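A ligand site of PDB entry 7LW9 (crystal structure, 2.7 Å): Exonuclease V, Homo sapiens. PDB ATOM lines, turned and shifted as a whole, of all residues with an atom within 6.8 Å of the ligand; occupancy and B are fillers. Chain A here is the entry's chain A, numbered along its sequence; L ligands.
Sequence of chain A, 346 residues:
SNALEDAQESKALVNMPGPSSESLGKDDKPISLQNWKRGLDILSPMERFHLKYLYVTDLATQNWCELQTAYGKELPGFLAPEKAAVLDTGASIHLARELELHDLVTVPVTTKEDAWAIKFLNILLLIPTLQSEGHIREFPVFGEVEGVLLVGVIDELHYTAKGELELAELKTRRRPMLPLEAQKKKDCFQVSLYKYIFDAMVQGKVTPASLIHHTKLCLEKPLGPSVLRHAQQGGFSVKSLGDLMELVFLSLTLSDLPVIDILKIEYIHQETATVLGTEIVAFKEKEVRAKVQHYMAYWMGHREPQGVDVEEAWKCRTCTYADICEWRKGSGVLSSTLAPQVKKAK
The side-chain sulfur of Cys 65 is bound to an iron atom (FE3) of the ligand, 2.7 Å away. A sulfur (S1) of the ligand lies close to the backbone NH (N) of Val 308 (3.7 Å). The side-chain amide nitrogen of Gln 68 lies close to a sulfur (S4) of the ligand. The backbone NH of Gln 68 lies close to a sulfur (S2) of the ligand. SG of Cys 319 binds FE1 of the ligand, at 2.7 Å.
The side-chain sulfur (SG) of Cys 65 lies close to the backbone NH (N) of Val 308, 3.8 Å away. O of Val 308 lies within hydrogen-bond range of NE1 of Trp 327 (2.9 Å). The backbone NH (N) of Trp 327 sits at hydrogen-bond distance from the side-chain sulfur (SG) of Cys 325, at 3.0 Å. The side-chain sulfur of Cys 319 lies close to the side-chain amide nitrogen of Gln 68, 3.5 Å away. The side-chain sulfur (SG) of Cys 316 lies within hydrogen-bond range of the backbone carbonyl oxygen (O) of Ala 313. The backbone NH of Leu 67 sits at hydrogen-bond distance from the backbone carbonyl oxygen of Gln 306, at 3.2 Å. The side-chain sulfur (SG) of Cys 319 lies close to the backbone NH (N) of Tyr 321. The side-chain sulfur (SG) of Cys 65 sits close to the backbone NH (N) of Gln 68 (3.7 Å).
Merely in contact with the ligand: Leu 67, Tyr 71, Gly 307, Cys 316, Ala 322, Cys 325 and Trp 327. Hydrophobic or aromatic side chains within 4 Å of the ligand: Leu 67, Tyr 71, Val 308 and Trp 327. 11 residues have an atom within 4 Å of the ligand: Cys 65, Leu 67, Gln 68, Tyr 71, Gly 307, Val 308, Cys 316, Cys 319, Ala 322, Cys 325 and Trp 327. The nearest printed residue that does not touch the ligand is Tyr 321 (4.2 Å).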
ATOM      1  N   TRP A  64      31.074 -20.211   0.757  1.00  0.00           N
ATOM      2  CA  TRP A  64      29.753 -20.403   0.189  1.00  0.00           C
ATOM      3  C   TRP A  64      28.720 -19.763   1.103  1.00  0.00           C
ATOM      4  O   TRP A  64      28.071 -18.776   0.739  1.00  0.00           O
ATOM      5  CB  TRP A  64      29.465 -21.898  -0.005  1.00  0.00           C
ATOM      6  CG  TRP A  64      28.113 -22.190  -0.572  1.00  0.00           C
ATOM      7  CD1 TRP A  64      27.001 -22.584   0.123  1.00  0.00           C
ATOM      8  CD2 TRP A  64      27.709 -22.119  -1.953  1.00  0.00           C
ATOM      9  NE1 TRP A  64      25.941 -22.759  -0.731  1.00  0.00           N
ATOM     10  CE2 TRP A  64      26.350 -22.479  -2.012  1.00  0.00           C
ATOM     11  CE3 TRP A  64      28.377 -21.779  -3.134  1.00  0.00           C
ATOM     12  CZ2 TRP A  64      25.648 -22.517  -3.217  1.00  0.00           C
ATOM     13  CZ3 TRP A  64      27.669 -21.816  -4.318  1.00  0.00           C
ATOM     14  CH2 TRP A  64      26.320 -22.184  -4.350  1.00  0.00           C
ATOM     15  N   CYS A  65      28.558 -20.324   2.294  1.00  0.00           N
ATOM     16  CA  CYS A  65      27.863 -19.630   3.376  1.00  0.00           C
ATOM     17  C   CYS A  65      28.460 -20.055   4.715  1.00  0.00           C
ATOM     18  O   CYS A  65      28.547 -21.246   5.015  1.00  0.00           O
ATOM     19  CB  CYS A  65      26.372 -19.905   3.388  1.00  0.00           C
ATOM     20  SG  CYS A  65      25.587 -18.936   4.685  1.00  0.00           S
ATOM     21  N   GLU A  66      28.824 -19.047   5.517  1.00  0.00           N
ATOM     22  CA  GLU A  66      29.466 -19.309   6.805  1.00  0.00           C
ATOM     23  C   GLU A  66      28.471 -19.884   7.808  1.00  0.00           C
ATOM     24  O   GLU A  66      28.814 -20.788   8.575  1.00  0.00           O
ATOM     25  CB  GLU A  66      30.098 -18.019   7.304  1.00  0.00           C
ATOM     26  CG  GLU A  66      30.640 -18.057   8.717  1.00  0.00           C
ATOM     27  CD  GLU A  66      31.321 -16.753   9.090  1.00  0.00           C
ATOM     28  OE1 GLU A  66      32.559 -16.738   9.238  1.00  0.00           O
ATOM     29  OE2 GLU A  66      30.615 -15.725   9.202  1.00  0.00           O
ATOM     30  N   LEU A  67      27.241 -19.366   7.820  1.00  0.00           N
ATOM     31  CA  LEU A  67      26.214 -19.902   8.699  1.00  0.00           C
ATOM     32  C   LEU A  67      25.939 -21.372   8.400  1.00  0.00           C
ATOM     33  O   LEU A  67      25.758 -22.179   9.327  1.00  0.00           O
ATOM     34  CB  LEU A  67      24.928 -19.082   8.549  1.00  0.00           C
ATOM     35  CG  LEU A  67      24.014 -18.894   9.756  1.00  0.00           C
ATOM     36  CD1 LEU A  67      24.789 -18.918  11.062  1.00  0.00           C
ATOM     37  CD2 LEU A  67      23.282 -17.590   9.615  1.00  0.00           C
ATOM     38  N   GLN A  68      25.908 -21.731   7.121  1.00  0.00           N
ATOM     39  CA  GLN A  68      25.683 -23.118   6.740  1.00  0.00           C
ATOM     40  C   GLN A  68      26.820 -24.019   7.199  1.00  0.00           C
ATOM     41  O   GLN A  68      26.582 -25.146   7.648  1.00  0.00           O
ATOM     42  CB  GLN A  68      25.504 -23.197   5.226  1.00  0.00           C
ATOM     43  CG  GLN A  68      24.916 -24.488   4.703  1.00  0.00           C
ATOM     44  CD  GLN A  68      24.953 -24.556   3.194  1.00  0.00           C
ATOM     45  OE1 GLN A  68      25.937 -24.993   2.609  1.00  0.00           O
ATOM     46  NE2 GLN A  68      23.885 -24.104   2.556  1.00  0.00           N
ATOM     47  N   THR A  69      28.061 -23.543   7.093  1.00  0.00           N
ATOM     48  CA  THR A  69      29.196 -24.298   7.614  1.00  0.00           C
ATOM     49  C   THR A  69      29.065 -24.514   9.119  1.00  0.00           C
ATOM     50  O   THR A  69      29.361 -25.600   9.633  1.00  0.00           O
ATOM     51  CB  THR A  69      30.497 -23.584   7.289  1.00  0.00           C
ATOM     52  OG1 THR A  69      30.646 -23.460   5.865  1.00  0.00           O
ATOM     53  CG2 THR A  69      31.697 -24.355   7.840  1.00  0.00           C
ATOM     54  N   TYR A  71      26.286 -24.642  10.918  1.00  0.00           N
ATOM     55  CA  TYR A  71      25.231 -25.607  11.203  1.00  0.00           C
ATOM     56  C   TYR A  71      25.683 -27.029  10.935  1.00  0.00           C
ATOM     57  O   TYR A  71      25.270 -27.959  11.651  1.00  0.00           O
ATOM     58  CB  TYR A  71      23.993 -25.290  10.360  1.00  0.00           C
ATOM     59  CG  TYR A  71      23.150 -24.144  10.888  1.00  0.00           C
ATOM     60  CD1 TYR A  71      22.776 -24.080  12.227  1.00  0.00           C
ATOM     61  CD2 TYR A  71      22.727 -23.135  10.034  1.00  0.00           C
ATOM     62  CE1 TYR A  71      22.004 -23.034  12.702  1.00  0.00           C
ATOM     63  CE2 TYR A  71      21.959 -22.086  10.502  1.00  0.00           C
ATOM     64  CZ  TYR A  71      21.596 -22.048  11.836  1.00  0.00           C
ATOM     65  OH  TYR A  71      20.830 -21.003  12.290  1.00  0.00           O
ATOM     66  N   GLN A 306      28.009 -15.025   9.710  1.00  0.00           N
ATOM     67  CA  GLN A 306      27.176 -14.304   8.769  1.00  0.00           C
ATOM     68  C   GLN A 306      26.548 -15.254   7.755  1.00  0.00           C
ATOM     69  O   GLN A 306      27.201 -16.189   7.283  1.00  0.00           O
ATOM     70  CB  GLN A 306      27.983 -13.238   8.017  1.00  0.00           C
ATOM     71  CG  GLN A 306      28.447 -12.070   8.883  1.00  0.00           C
ATOM     72  CD  GLN A 306      29.318 -11.090   8.119  1.00  0.00           C
ATOM     73  OE1 GLN A 306      29.159 -10.914   6.911  1.00  0.00           O
ATOM     74  NE2 GLN A 306      30.240 -10.449   8.824  1.00  0.00           N
ATOM     75  N   GLY A 307      25.284 -15.007   7.433  1.00  0.00           N
ATOM     76  CA  GLY A 307      24.603 -15.729   6.376  1.00  0.00           C
ATOM     77  C   GLY A 307      24.949 -15.157   5.012  1.00  0.00           C
ATOM     78  O   GLY A 307      25.896 -14.386   4.841  1.00  0.00           O
ATOM     79  N   VAL A 308      24.145 -15.537   4.020  1.00  0.00           N
ATOM     80  CA  VAL A 308      24.374 -15.102   2.641  1.00  0.00           C
ATOM     81  C   VAL A 308      23.905 -13.666   2.462  1.00  0.00           C
ATOM     82  O   VAL A 308      23.002 -13.181   3.163  1.00  0.00           O
ATOM     83  CB  VAL A 308      23.682 -16.035   1.634  1.00  0.00           C
ATOM     84  CG1 VAL A 308      24.280 -17.423   1.686  1.00  0.00           C
ATOM     85  CG2 VAL A 308      22.173 -16.070   1.900  1.00  0.00           C
ATOM     86  N   GLU A 312      22.420 -13.241  -3.026  1.00  0.00           N
ATOM     87  CA  GLU A 312      22.637 -14.673  -3.174  1.00  0.00           C
ATOM     88  C   GLU A 312      21.653 -15.488  -2.341  1.00  0.00           C
ATOM     89  O   GLU A 312      21.962 -16.589  -1.888  1.00  0.00           O
ATOM     90  CB  GLU A 312      24.076 -15.039  -2.791  1.00  0.00           C
ATOM     91  CG  GLU A 312      25.060 -14.977  -3.948  1.00  0.00           C
ATOM     92  CD  GLU A 312      26.500 -15.120  -3.493  1.00  0.00           C
ATOM     93  OE1 GLU A 312      26.807 -14.690  -2.357  1.00  0.00           O
ATOM     94  OE2 GLU A 312      27.325 -15.659  -4.262  1.00  0.00           O
ATOM     95  N   ALA A 313      20.438 -14.955  -2.143  1.00  0.00           N
ATOM     96  CA  ALA A 313      19.417 -15.659  -1.370  1.00  0.00           C
ATOM     97  C   ALA A 313      18.959 -16.947  -2.026  1.00  0.00           C
ATOM     98  O   ALA A 313      18.250 -17.729  -1.391  1.00  0.00           O
ATOM     99  CB  ALA A 313      18.217 -14.742  -1.132  1.00  0.00           C
ATOM    100  N   LYS A 315      20.841 -19.380  -2.661  1.00  0.00           N
ATOM    101  CA  LYS A 315      21.545 -20.466  -1.988  1.00  0.00           C
ATOM    102  C   LYS A 315      20.675 -21.121  -0.923  1.00  0.00           C
ATOM    103  O   LYS A 315      20.845 -22.313  -0.625  1.00  0.00           O
ATOM    104  CB  LYS A 315      22.838 -19.946  -1.344  1.00  0.00           C
ATOM    105  CG  LYS A 315      23.897 -19.457  -2.323  1.00  0.00           C
ATOM    106  CD  LYS A 315      25.146 -19.016  -1.567  1.00  0.00           C
ATOM    107  CE  LYS A 315      26.194 -18.429  -2.498  1.00  0.00           C
ATOM    108  NZ  LYS A 315      27.361 -17.893  -1.735  1.00  0.00           N
ATOM    109  N   CYS A 316      19.734 -20.372  -0.351  1.00  0.00           N
ATOM    110  CA  CYS A 316      18.898 -20.889   0.731  1.00  0.00           C
ATOM    111  C   CYS A 316      17.851 -21.866   0.240  1.00  0.00           C
ATOM    112  O   CYS A 316      17.342 -22.664   1.032  1.00  0.00           O
ATOM    113  CB  CYS A 316      18.206 -19.721   1.440  1.00  0.00           C
ATOM    114  SG  CYS A 316      19.147 -18.187   1.520  1.00  0.00           S
ATOM    115  N   ARG A 317      17.505 -21.807  -1.052  1.00  0.00           N
ATOM    116  CA  ARG A 317      16.455 -22.667  -1.592  1.00  0.00           C
ATOM    117  C   ARG A 317      16.800 -24.139  -1.487  1.00  0.00           C
ATOM    118  O   ARG A 317      15.902 -24.983  -1.541  1.00  0.00           O
ATOM    119  CB  ARG A 317      16.180 -22.296  -3.053  1.00  0.00           C
ATOM    120  CG  ARG A 317      14.774 -22.648  -3.554  1.00  0.00           C
ATOM    121  CD  ARG A 317      14.779 -23.926  -4.372  1.00  0.00           C
ATOM    122  NE  ARG A 317      15.643 -23.836  -5.549  1.00  0.00           N
ATOM    123  CZ  ARG A 317      15.955 -24.855  -6.337  1.00  0.00           C
ATOM    124  NH1 ARG A 317      16.739 -24.681  -7.389  1.00  0.00           N
ATOM    125  NH2 ARG A 317      15.458 -26.058  -6.082  1.00  0.00           N
ATOM    126  N   THR A 318      18.083 -24.475  -1.328  1.00  0.00           N
ATOM    127  CA  THR A 318      18.538 -25.854  -1.293  1.00  0.00           C
ATOM    128  C   THR A 318      19.295 -26.189  -0.008  1.00  0.00           C
ATOM    129  O   THR A 318      19.938 -27.239   0.067  1.00  0.00           O
ATOM    130  CB  THR A 318      19.408 -26.171  -2.506  1.00  0.00           C
ATOM    131  OG1 THR A 318      20.283 -25.058  -2.756  1.00  0.00           O
ATOM    132  CG2 THR A 318      18.551 -26.425  -3.733  1.00  0.00           C
ATOM    133  N   CYS A 319      19.227 -25.326   1.001  1.00  0.00           N
ATOM    134  CA  CYS A 319      19.997 -25.550   2.219  1.00  0.00           C
ATOM    135  C   CYS A 319      19.248 -26.474   3.163  1.00  0.00           C
ATOM    136  O   CYS A 319      18.055 -26.268   3.443  1.00  0.00           O
ATOM    137  CB  CYS A 319      20.301 -24.230   2.924  1.00  0.00           C
ATOM    138  SG  CYS A 319      21.055 -24.521   4.534  1.00  0.00           S
ATOM    139  N   THR A 320      19.937 -27.504   3.655  1.00  0.00           N
ATOM    140  CA  THR A 320      19.372 -28.410   4.651  1.00  0.00           C
ATOM    141  C   THR A 320      18.819 -27.648   5.844  1.00  0.00           C
ATOM    142  O   THR A 320      17.751 -27.977   6.370  1.00  0.00           O
ATOM    143  CB  THR A 320      20.445 -29.410   5.106  1.00  0.00           C
ATOM    144  OG1 THR A 320      21.276 -29.762   3.990  1.00  0.00           O
ATOM    145  CG2 THR A 320      19.806 -30.653   5.680  1.00  0.00           C
ATOM    146  N   TYR A 321      19.529 -26.602   6.282  1.00  0.00           N
ATOM    147  CA  TYR A 321      19.175 -25.845   7.476  1.00  0.00           C
ATOM    148  C   TYR A 321      18.326 -24.610   7.153  1.00  0.00           C
ATOM    149  O   TYR A 321      18.419 -23.607   7.871  1.00  0.00           O
ATOM    150  CB  TYR A 321      20.441 -25.442   8.226  1.00  0.00           C
ATOM    151  CG  TYR A 321      21.445 -26.576   8.324  1.00  0.00           C
ATOM    152  CD1 TYR A 321      21.265 -27.608   9.240  1.00  0.00           C
ATOM    153  CD2 TYR A 321      22.558 -26.621   7.490  1.00  0.00           C
ATOM    154  CE1 TYR A 321      22.168 -28.646   9.334  1.00  0.00           C
ATOM    155  CE2 TYR A 321      23.474 -27.660   7.579  1.00  0.00           C
ATOM    156  CZ  TYR A 321      23.269 -28.666   8.505  1.00  0.00           C
ATOM    157  OH  TYR A 321      24.177 -29.700   8.591  1.00  0.00           O
ATOM    158  N   ALA A 322      17.497 -24.671   6.111  1.00  0.00           N
ATOM    159  CA  ALA A 322      16.708 -23.515   5.727  1.00  0.00           C
ATOM    160  C   ALA A 322      15.558 -23.259   6.692  1.00  0.00           C
ATOM    161  O   ALA A 322      15.181 -22.100   6.914  1.00  0.00           O
ATOM    162  CB  ALA A 322      16.177 -23.683   4.305  1.00  0.00           C
ATOM    163  N   ASP A 323      14.972 -24.313   7.268  1.00  0.00           N
ATOM    164  CA  ASP A 323      13.833 -24.125   8.161  1.00  0.00           C
ATOM    165  C   ASP A 323      14.251 -23.641   9.543  1.00  0.00           C
ATOM    166  O   ASP A 323      13.521 -22.867  10.160  1.00  0.00           O
ATOM    167  CB  ASP A 323      13.037 -25.429   8.263  1.00  0.00           C
ATOM    168  CG  ASP A 323      13.930 -26.656   8.332  1.00  0.00           C
ATOM    169  OD1 ASP A 323      15.160 -26.503   8.302  1.00  0.00           O
ATOM    170  OD2 ASP A 323      13.382 -27.780   8.408  1.00  0.00           O
ATOM    171  N   CYS A 325      16.994 -21.840  10.289  1.00  0.00           N
ATOM    172  CA  CYS A 325      17.810 -20.632  10.292  1.00  0.00           C
ATOM    173  C   CYS A 325      16.978 -19.404  10.603  1.00  0.00           C
ATOM    174  O   CYS A 325      15.777 -19.337  10.301  1.00  0.00           O
ATOM    175  CB  CYS A 325      18.511 -20.468   8.943  1.00  0.00           C
ATOM    176  SG  CYS A 325      19.341 -18.878   8.774  1.00  0.00           S
ATOM    177  N   GLU A 326      17.629 -18.406  11.208  1.00  0.00           N
ATOM    178  CA  GLU A 326      17.004 -17.130  11.510  1.00  0.00           C
ATOM    179  C   GLU A 326      17.615 -15.969  10.749  1.00  0.00           C
ATOM    180  O   GLU A 326      17.154 -14.837  10.899  1.00  0.00           O
ATOM    181  CB  GLU A 326      17.059 -16.847  13.017  1.00  0.00           C
ATOM    182  CG  GLU A 326      15.749 -16.347  13.614  1.00  0.00           C
ATOM    183  CD  GLU A 326      15.556 -14.850  13.447  1.00  0.00           C
ATOM    184  OE1 GLU A 326      16.491 -14.093  13.779  1.00  0.00           O
ATOM    185  OE2 GLU A 326      14.482 -14.437  12.974  1.00  0.00           O
ATOM    186  N   TRP A 327      18.656 -16.217   9.946  1.00  0.00           N
ATOM    187  CA  TRP A 327      19.256 -15.142   9.153  1.00  0.00           C
ATOM    188  C   TRP A 327      18.362 -14.799   7.966  1.00  0.00           C
ATOM    189  O   TRP A 327      18.073 -13.622   7.717  1.00  0.00           O
ATOM    190  CB  TRP A 327      20.642 -15.557   8.673  1.00  0.00           C
ATOM    191  CG  TRP A 327      21.283 -14.606   7.703  1.00  0.00           C
ATOM    192  CD1 TRP A 327      21.033 -14.510   6.359  1.00  0.00           C
ATOM    193  CD2 TRP A 327      22.286 -13.637   7.993  1.00  0.00           C
ATOM    194  NE1 TRP A 327      21.819 -13.533   5.803  1.00  0.00           N
ATOM    195  CE2 TRP A 327      22.601 -12.980   6.783  1.00  0.00           C
ATOM    196  CE3 TRP A 327      22.949 -13.249   9.166  1.00  0.00           C
ATOM    197  CZ2 TRP A 327      23.543 -11.955   6.718  1.00  0.00           C
ATOM    198  CZ3 TRP A 327      23.899 -12.242   9.086  1.00  0.00           C
ATOM    199  CH2 TRP A 327      24.179 -11.607   7.871  1.00  0.00           C
ATOM    200  N   ARG A 328      17.932 -15.813   7.209  1.00  0.00           N
ATOM    201  CA  ARG A 328      17.159 -15.569   5.999  1.00  0.00           C
ATOM    202  C   ARG A 328      15.838 -14.869   6.319  1.00  0.00           C
ATOM    203  O   ARG A 328      15.389 -14.012   5.546  1.00  0.00           O
ATOM    204  CB  ARG A 328      16.907 -16.892   5.273  1.00  0.00           C
ATOM    205  CG  ARG A 328      16.006 -16.783   4.054  1.00  0.00           C
ATOM    206  CD  ARG A 328      15.609 -18.158   3.567  1.00  0.00           C
ATOM    207  NE  ARG A 328      14.195 -18.430   3.809  1.00  0.00           N
ATOM    208  CZ  ARG A 328      13.499 -19.373   3.177  1.00  0.00           C
ATOM    209  NH1 ARG A 328      12.218 -19.562   3.471  1.00  0.00           N
ATOM    210  NH2 ARG A 328      14.087 -20.136   2.263  1.00  0.00           N
HETATM  211 FE1  LIG L   1      21.257 -21.827   4.788  1.00  0.00          FE
HETATM  212 FE2  LIG L   1      20.649 -19.399   3.690  1.00  0.00          FE
HETATM  213 FE3  LIG L   1      23.057 -19.782   4.927  1.00  0.00          FE
HETATM  214 FE4  LIG L   1      20.780 -19.683   6.410  1.00  0.00          FE
HETATM  215  S1  LIG L   1      21.669 -18.000   5.171  1.00  0.00           S
HETATM  216  S2  LIG L   1      22.469 -21.194   6.615  1.00  0.00           S
HETATM  217  S3  LIG L   1      19.298 -20.689   4.994  1.00  0.00           S
HETATM  218  S4  LIG L   1      22.304 -20.816   3.031  1.00  0.00           S
